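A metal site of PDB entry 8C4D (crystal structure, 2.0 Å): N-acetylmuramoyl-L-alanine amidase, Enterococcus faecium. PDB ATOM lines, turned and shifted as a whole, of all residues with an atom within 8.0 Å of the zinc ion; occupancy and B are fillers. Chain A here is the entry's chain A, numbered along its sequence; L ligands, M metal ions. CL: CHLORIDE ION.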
ATOM      1  N   VAL A  25      14.512 -26.679   9.918  1.00  0.00           N
ATOM      2  CA  VAL A  25      14.956 -26.744  11.314  1.00  0.00           C
ATOM      3  C   VAL A  25      14.805 -25.362  11.906  1.00  0.00           C
ATOM      4  O   VAL A  25      15.311 -24.386  11.345  1.00  0.00           O
ATOM      5  CB  VAL A  25      16.412 -27.234  11.435  1.00  0.00           C
ATOM      6  CG1 VAL A  25      16.882 -27.188  12.894  1.00  0.00           C
ATOM      7  CG2 VAL A  25      16.575 -28.636  10.847  1.00  0.00           C
ATOM      8  N   ILE A  26      14.082 -25.267  13.020  1.00  0.00           N
ATOM      9  CA  ILE A  26      13.899 -23.990  13.707  1.00  0.00           C
ATOM     10  C   ILE A  26      14.949 -23.911  14.809  1.00  0.00           C
ATOM     11  O   ILE A  26      14.883 -24.675  15.784  1.00  0.00           O
ATOM     12  CB  ILE A  26      12.481 -23.850  14.296  1.00  0.00           C
ATOM     13  CG1 ILE A  26      11.393 -24.150  13.255  1.00  0.00           C
ATOM     14  CG2 ILE A  26      12.318 -22.445  14.874  1.00  0.00           C
ATOM     15  CD1 ILE A  26      11.340 -23.158  12.065  1.00  0.00           C
ATOM     16  N   HIS A  27      15.890 -22.978  14.671  1.00  0.00           N
ATOM     17  CA  HIS A  27      16.942 -22.704  15.642  1.00  0.00           C
ATOM     18  C   HIS A  27      16.599 -21.463  16.464  1.00  0.00           C
ATOM     19  O   HIS A  27      15.758 -20.643  16.093  1.00  0.00           O
ATOM     20  CB  HIS A  27      18.312 -22.457  14.968  1.00  0.00           C
ATOM     21  CG  HIS A  27      18.751 -23.515  13.990  1.00  0.00           C
ATOM     22  ND1 HIS A  27      19.660 -24.493  14.315  1.00  0.00           N
ATOM     23  CD2 HIS A  27      18.471 -23.685  12.671  1.00  0.00           C
ATOM     24  CE1 HIS A  27      19.897 -25.247  13.260  1.00  0.00           C
ATOM     25  NE2 HIS A  27      19.181 -24.782  12.253  1.00  0.00           N
ATOM     26  N   ASN A  28      17.307 -21.295  17.594  1.00  0.00           N
ATOM     27  CA  ASN A  28      17.416 -20.019  18.289  1.00  0.00           C
ATOM     28  C   ASN A  28      18.881 -19.614  18.328  1.00  0.00           C
ATOM     29  O   ASN A  28      19.757 -20.445  18.571  1.00  0.00           O
ATOM     30  CB  ASN A  28      16.901 -20.073  19.744  1.00  0.00           C
ATOM     31  CG  ASN A  28      15.475 -20.611  19.886  1.00  0.00           C
ATOM     32  OD1 ASN A  28      15.084 -21.000  20.993  1.00  0.00           O
ATOM     33  ND2 ASN A  28      14.663 -20.568  18.818  1.00  0.00           N
ATOM     34  N   THR A  29      19.163 -18.322  18.141  1.00  0.00           N
ATOM     35  CA  THR A  29      20.558 -17.902  18.102  1.00  0.00           C
ATOM     36  C   THR A  29      21.236 -17.992  19.458  1.00  0.00           C
ATOM     37  O   THR A  29      22.477 -18.045  19.510  1.00  0.00           O
ATOM     38  CB  THR A  29      20.680 -16.460  17.626  1.00  0.00           C
ATOM     39  OG1 THR A  29      19.993 -15.604  18.557  1.00  0.00           O
ATOM     40  CG2 THR A  29      20.086 -16.293  16.219  1.00  0.00           C
ATOM     41  N   TRP A  30      20.476 -18.016  20.538  1.00  0.00           N
ATOM     42  CA  TRP A  30      21.015 -17.837  21.890  1.00  0.00           C
ATOM     43  C   TRP A  30      21.910 -16.600  21.945  1.00  0.00           C
ATOM     44  O   TRP A  30      22.967 -16.586  22.590  1.00  0.00           O
ATOM     45  CB  TRP A  30      21.758 -19.090  22.375  1.00  0.00           C
ATOM     46  CG  TRP A  30      21.765 -19.155  23.887  1.00  0.00           C
ATOM     47  CD1 TRP A  30      22.863 -19.082  24.706  1.00  0.00           C
ATOM     48  CD2 TRP A  30      20.619 -19.273  24.743  1.00  0.00           C
ATOM     49  NE1 TRP A  30      22.473 -19.145  26.023  1.00  0.00           N
ATOM     50  CE2 TRP A  30      21.106 -19.262  26.078  1.00  0.00           C
ATOM     51  CE3 TRP A  30      19.238 -19.384  24.519  1.00  0.00           C
ATOM     52  CZ2 TRP A  30      20.254 -19.378  27.183  1.00  0.00           C
ATOM     53  CZ3 TRP A  30      18.395 -19.489  25.628  1.00  0.00           C
ATOM     54  CH2 TRP A  30      18.903 -19.480  26.941  1.00  0.00           C
ATOM     55  N   ALA A  55      23.084 -20.346   9.021  1.00  0.00           N
ATOM     56  CA  ALA A  55      21.764 -20.792   8.605  1.00  0.00           C
ATOM     57  C   ALA A  55      21.325 -20.034   7.349  1.00  0.00           C
ATOM     58  O   ALA A  55      22.004 -19.107   6.877  1.00  0.00           O
ATOM     59  CB  ALA A  55      20.726 -20.577   9.725  1.00  0.00           C
ATOM     60  N   HIS A  76      24.369 -25.753   9.300  1.00  0.00           N
ATOM     61  CA  HIS A  76      23.573 -25.350  10.442  1.00  0.00           C
ATOM     62  C   HIS A  76      23.306 -26.422  11.495  1.00  0.00           C
ATOM     63  O   HIS A  76      22.887 -26.059  12.603  1.00  0.00           O
ATOM     64  CB  HIS A  76      22.224 -24.748   9.978  1.00  0.00           C
ATOM     65  CG  HIS A  76      21.307 -25.704   9.276  1.00  0.00           C
ATOM     66  ND1 HIS A  76      20.048 -25.995   9.749  1.00  0.00           N
ATOM     67  CD2 HIS A  76      21.438 -26.372   8.101  1.00  0.00           C
ATOM     68  CE1 HIS A  76      19.442 -26.822   8.906  1.00  0.00           C
ATOM     69  NE2 HIS A  76      20.269 -27.065   7.904  1.00  0.00           N
ATOM     70  N   VAL A  77      23.539 -27.709  11.222  1.00  0.00           N
ATOM     71  CA  VAL A  77      23.235 -28.713  12.243  1.00  0.00           C
ATOM     72  C   VAL A  77      24.333 -29.741  12.490  1.00  0.00           C
ATOM     73  O   VAL A  77      24.096 -30.728  13.192  1.00  0.00           O
ATOM     74  CB  VAL A  77      21.936 -29.481  11.931  1.00  0.00           C
ATOM     75  CG1 VAL A  77      20.701 -28.585  12.083  1.00  0.00           C
ATOM     76  CG2 VAL A  77      22.020 -30.127  10.554  1.00  0.00           C
ATOM     77  N   TYR A  89      16.449 -21.966   9.994  1.00  0.00           N
ATOM     78  CA  TYR A  89      15.861 -20.676  10.374  1.00  0.00           C
ATOM     79  C   TYR A  89      16.340 -20.317  11.768  1.00  0.00           C
ATOM     80  O   TYR A  89      16.112 -21.064  12.728  1.00  0.00           O
ATOM     81  CB  TYR A  89      14.310 -20.740  10.352  1.00  0.00           C
ATOM     82  CG  TYR A  89      13.763 -21.139   8.998  1.00  0.00           C
ATOM     83  CD1 TYR A  89      13.802 -22.458   8.581  1.00  0.00           C
ATOM     84  CD2 TYR A  89      13.244 -20.186   8.122  1.00  0.00           C
ATOM     85  CE1 TYR A  89      13.342 -22.838   7.337  1.00  0.00           C
ATOM     86  CE2 TYR A  89      12.763 -20.559   6.849  1.00  0.00           C
ATOM     87  CZ  TYR A  89      12.822 -21.888   6.470  1.00  0.00           C
ATOM     88  OH  TYR A  89      12.374 -22.298   5.228  1.00  0.00           O
ATOM     89  N   GLU A  90      17.011 -19.170  11.903  1.00  0.00           N
ATOM     90  CA  GLU A  90      17.567 -18.745  13.170  1.00  0.00           C
ATOM     91  C   GLU A  90      16.664 -17.670  13.770  1.00  0.00           C
ATOM     92  O   GLU A  90      16.421 -16.641  13.134  1.00  0.00           O
ATOM     93  CB  GLU A  90      18.994 -18.211  13.007  1.00  0.00           C
ATOM     94  CG  GLU A  90      20.084 -19.279  12.920  1.00  0.00           C
ATOM     95  CD  GLU A  90      20.473 -19.875  14.285  1.00  0.00           C
ATOM     96  OE1 GLU A  90      21.358 -20.746  14.308  1.00  0.00           O
ATOM     97  OE2 GLU A  90      19.872 -19.491  15.317  1.00  0.00           O
ATOM     98  N   CYS A 131      14.130 -30.170  15.109  1.00  0.00           N
ATOM     99  CA  CYS A 131      14.994 -29.427  16.020  1.00  0.00           C
ATOM    100  C   CYS A 131      16.465 -29.777  15.776  1.00  0.00           C
ATOM    101  O   CYS A 131      16.794 -30.893  15.386  1.00  0.00           O
ATOM    102  CB  CYS A 131      14.636 -29.736  17.473  1.00  0.00           C
ATOM    103  SG  CYS A 131      12.917 -29.286  17.925  1.00  0.00           S
ATOM    104  N   HIS A 132      17.331 -28.793  16.007  1.00  0.00           N
ATOM    105  CA  HIS A 132      18.772 -28.973  15.854  1.00  0.00           C
ATOM    106  C   HIS A 132      19.262 -30.187  16.644  1.00  0.00           C
ATOM    107  O   HIS A 132      20.044 -30.997  16.132  1.00  0.00           O
ATOM    108  CB  HIS A 132      19.470 -27.681  16.291  1.00  0.00           C
ATOM    109  CG  HIS A 132      20.951 -27.656  16.094  1.00  0.00           C
ATOM    110  ND1 HIS A 132      21.681 -26.488  16.182  1.00  0.00           N
ATOM    111  CD2 HIS A 132      21.855 -28.640  15.865  1.00  0.00           C
ATOM    112  CE1 HIS A 132      22.962 -26.757  15.983  1.00  0.00           C
ATOM    113  NE2 HIS A 132      23.094 -28.061  15.799  1.00  0.00           N
ATOM    114  N   HIS A 133      18.766 -30.372  17.873  1.00  0.00           N
ATOM    115  CA  HIS A 133      19.252 -31.473  18.706  1.00  0.00           C
ATOM    116  C   HIS A 133      18.796 -32.850  18.222  1.00  0.00           C
ATOM    117  O   HIS A 133      19.239 -33.854  18.781  1.00  0.00           O
ATOM    118  CB  HIS A 133      18.819 -31.255  20.157  1.00  0.00           C
ATOM    119  CG  HIS A 133      17.330 -31.306  20.368  1.00  0.00           C
ATOM    120  ND1 HIS A 133      16.573 -30.164  20.507  1.00  0.00           N
ATOM    121  CD2 HIS A 133      16.471 -32.340  20.455  1.00  0.00           C
ATOM    122  CE1 HIS A 133      15.307 -30.505  20.684  1.00  0.00           C
ATOM    123  NE2 HIS A 133      15.214 -31.817  20.655  1.00  0.00           N
ATOM    124  N   SER A 136      22.338 -33.391  16.100  1.00  0.00           N
ATOM    125  CA  SER A 136      23.617 -33.392  16.812  1.00  0.00           C
ATOM    126  C   SER A 136      23.380 -32.819  18.200  1.00  0.00           C
ATOM    127  O   SER A 136      22.344 -32.222  18.483  1.00  0.00           O
ATOM    128  CB  SER A 136      24.681 -32.605  16.037  1.00  0.00           C
ATOM    129  OG  SER A 136      24.264 -31.260  15.828  1.00  0.00           O
ATOM    130  N   THR A 138      23.082 -30.640  21.203  1.00  0.00           N
ATOM    131  CA  THR A 138      22.946 -29.221  21.493  1.00  0.00           C
ATOM    132  C   THR A 138      21.718 -29.050  22.372  1.00  0.00           C
ATOM    133  O   THR A 138      20.875 -29.949  22.467  1.00  0.00           O
ATOM    134  CB  THR A 138      22.790 -28.373  20.220  1.00  0.00           C
ATOM    135  OG1 THR A 138      22.576 -27.001  20.570  1.00  0.00           O
ATOM    136  CG2 THR A 138      21.595 -28.864  19.395  1.00  0.00           C
ATOM    137  N   GLU A 139      21.649 -27.884  23.015  1.00  0.00           N
ATOM    138  CA  GLU A 139      20.466 -27.432  23.736  1.00  0.00           C
ATOM    139  C   GLU A 139      19.467 -26.695  22.841  1.00  0.00           C
ATOM    140  O   GLU A 139      18.366 -26.391  23.310  1.00  0.00           O
ATOM    141  CB  GLU A 139      20.903 -26.514  24.887  1.00  0.00           C
ATOM    142  CG  GLU A 139      22.022 -27.134  25.753  1.00  0.00           C
ATOM    143  CD  GLU A 139      22.356 -26.316  26.991  1.00  0.00           C
ATOM    144  OE1 GLU A 139      21.483 -25.604  27.515  1.00  0.00           O
ATOM    145  OE2 GLU A 139      23.520 -26.406  27.459  1.00  0.00           O
ATOM    146  N   CYS A 140      19.841 -26.403  21.591  1.00  0.00           N
ATOM    147  CA  CYS A 140      18.990 -25.642  20.671  1.00  0.00           C
ATOM    148  C   CYS A 140      17.746 -26.447  20.327  1.00  0.00           C
ATOM    149  O   CYS A 140      17.808 -27.673  20.208  1.00  0.00           O
ATOM    150  CB  CYS A 140      19.803 -25.302  19.391  1.00  0.00           C
ATOM    151  SG  CYS A 140      18.988 -24.300  18.052  1.00  0.00           S
ATOM    152  N   PRO A 141      16.565 -25.787  20.160  1.00  0.00           N
ATOM    153  CA  PRO A 141      16.269 -24.344  20.271  1.00  0.00           C
ATOM    154  C   PRO A 141      15.911 -23.969  21.715  1.00  0.00           C
ATOM    155  O   PRO A 141      14.774 -24.175  22.160  1.00  0.00           O
ATOM    156  CB  PRO A 141      15.099 -24.163  19.308  1.00  0.00           C
ATOM    157  CG  PRO A 141      14.375 -25.508  19.293  1.00  0.00           C
ATOM    158  CD  PRO A 141      15.356 -26.552  19.838  1.00  0.00           C
ATOM    159  N   LYS A 142      16.857 -23.393  22.442  1.00  0.00           N
ATOM    160  CA  LYS A 142      16.757 -23.379  23.895  1.00  0.00           C
ATOM    161  C   LYS A 142      15.660 -22.440  24.382  1.00  0.00           C
ATOM    162  O   LYS A 142      14.890 -22.801  25.281  1.00  0.00           O
ATOM    163  CB  LYS A 142      18.109 -22.998  24.510  1.00  0.00           C
ATOM    164  CG  LYS A 142      18.086 -22.964  26.031  1.00  0.00           C
ATOM    165  CD  LYS A 142      19.482 -23.002  26.628  1.00  0.00           C
ATOM    166  CE  LYS A 142      19.427 -23.142  28.161  1.00  0.00           C
ATOM    167  NZ  LYS A 142      19.028 -24.521  28.562  1.00  0.00           N
HETATM  168 CL    CL L   1      22.223 -22.388  16.669  1.00  0.00          CL
HETATM  169 ZN    ZN M   1      20.540 -24.573  16.361  1.00  0.00          ZN
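A ring nitrogen (NE2) of His 27 lies within hydrogen-bond range of a ring nitrogen (ND1) of His 76 (2.9 Å).
N of His 27 lies within hydrogen-bond range of O of Tyr 89 (2.7 Å).
NE2 of His 132 is in hydrogen-bond range of OG of Ser 136, 3.4 Å away.
N of Asn 28 lies close to SG of Cys 140, at 3.5 Å.
The backbone NH of Cys 140 sits at hydrogen-bond distance from the side-chain hydroxyl of Thr 138 (3.0 Å).
O of Cys 140 is in hydrogen-bond range of ND1 of His 133.
The nearest printed residue that does not touch the zinc ion is Glu 90 (4.4 Å).
A ring nitrogen (ND1) of His 27 is bound to the zinc ion.
ND1 of His 132 binds the zinc ion (2.2 Å).
The zinc ion is bound by the side-chain sulfur (SG) of Cys 140 (2.3 Å).
CL of the ligand binds the zinc ion, 2.8 Å away.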
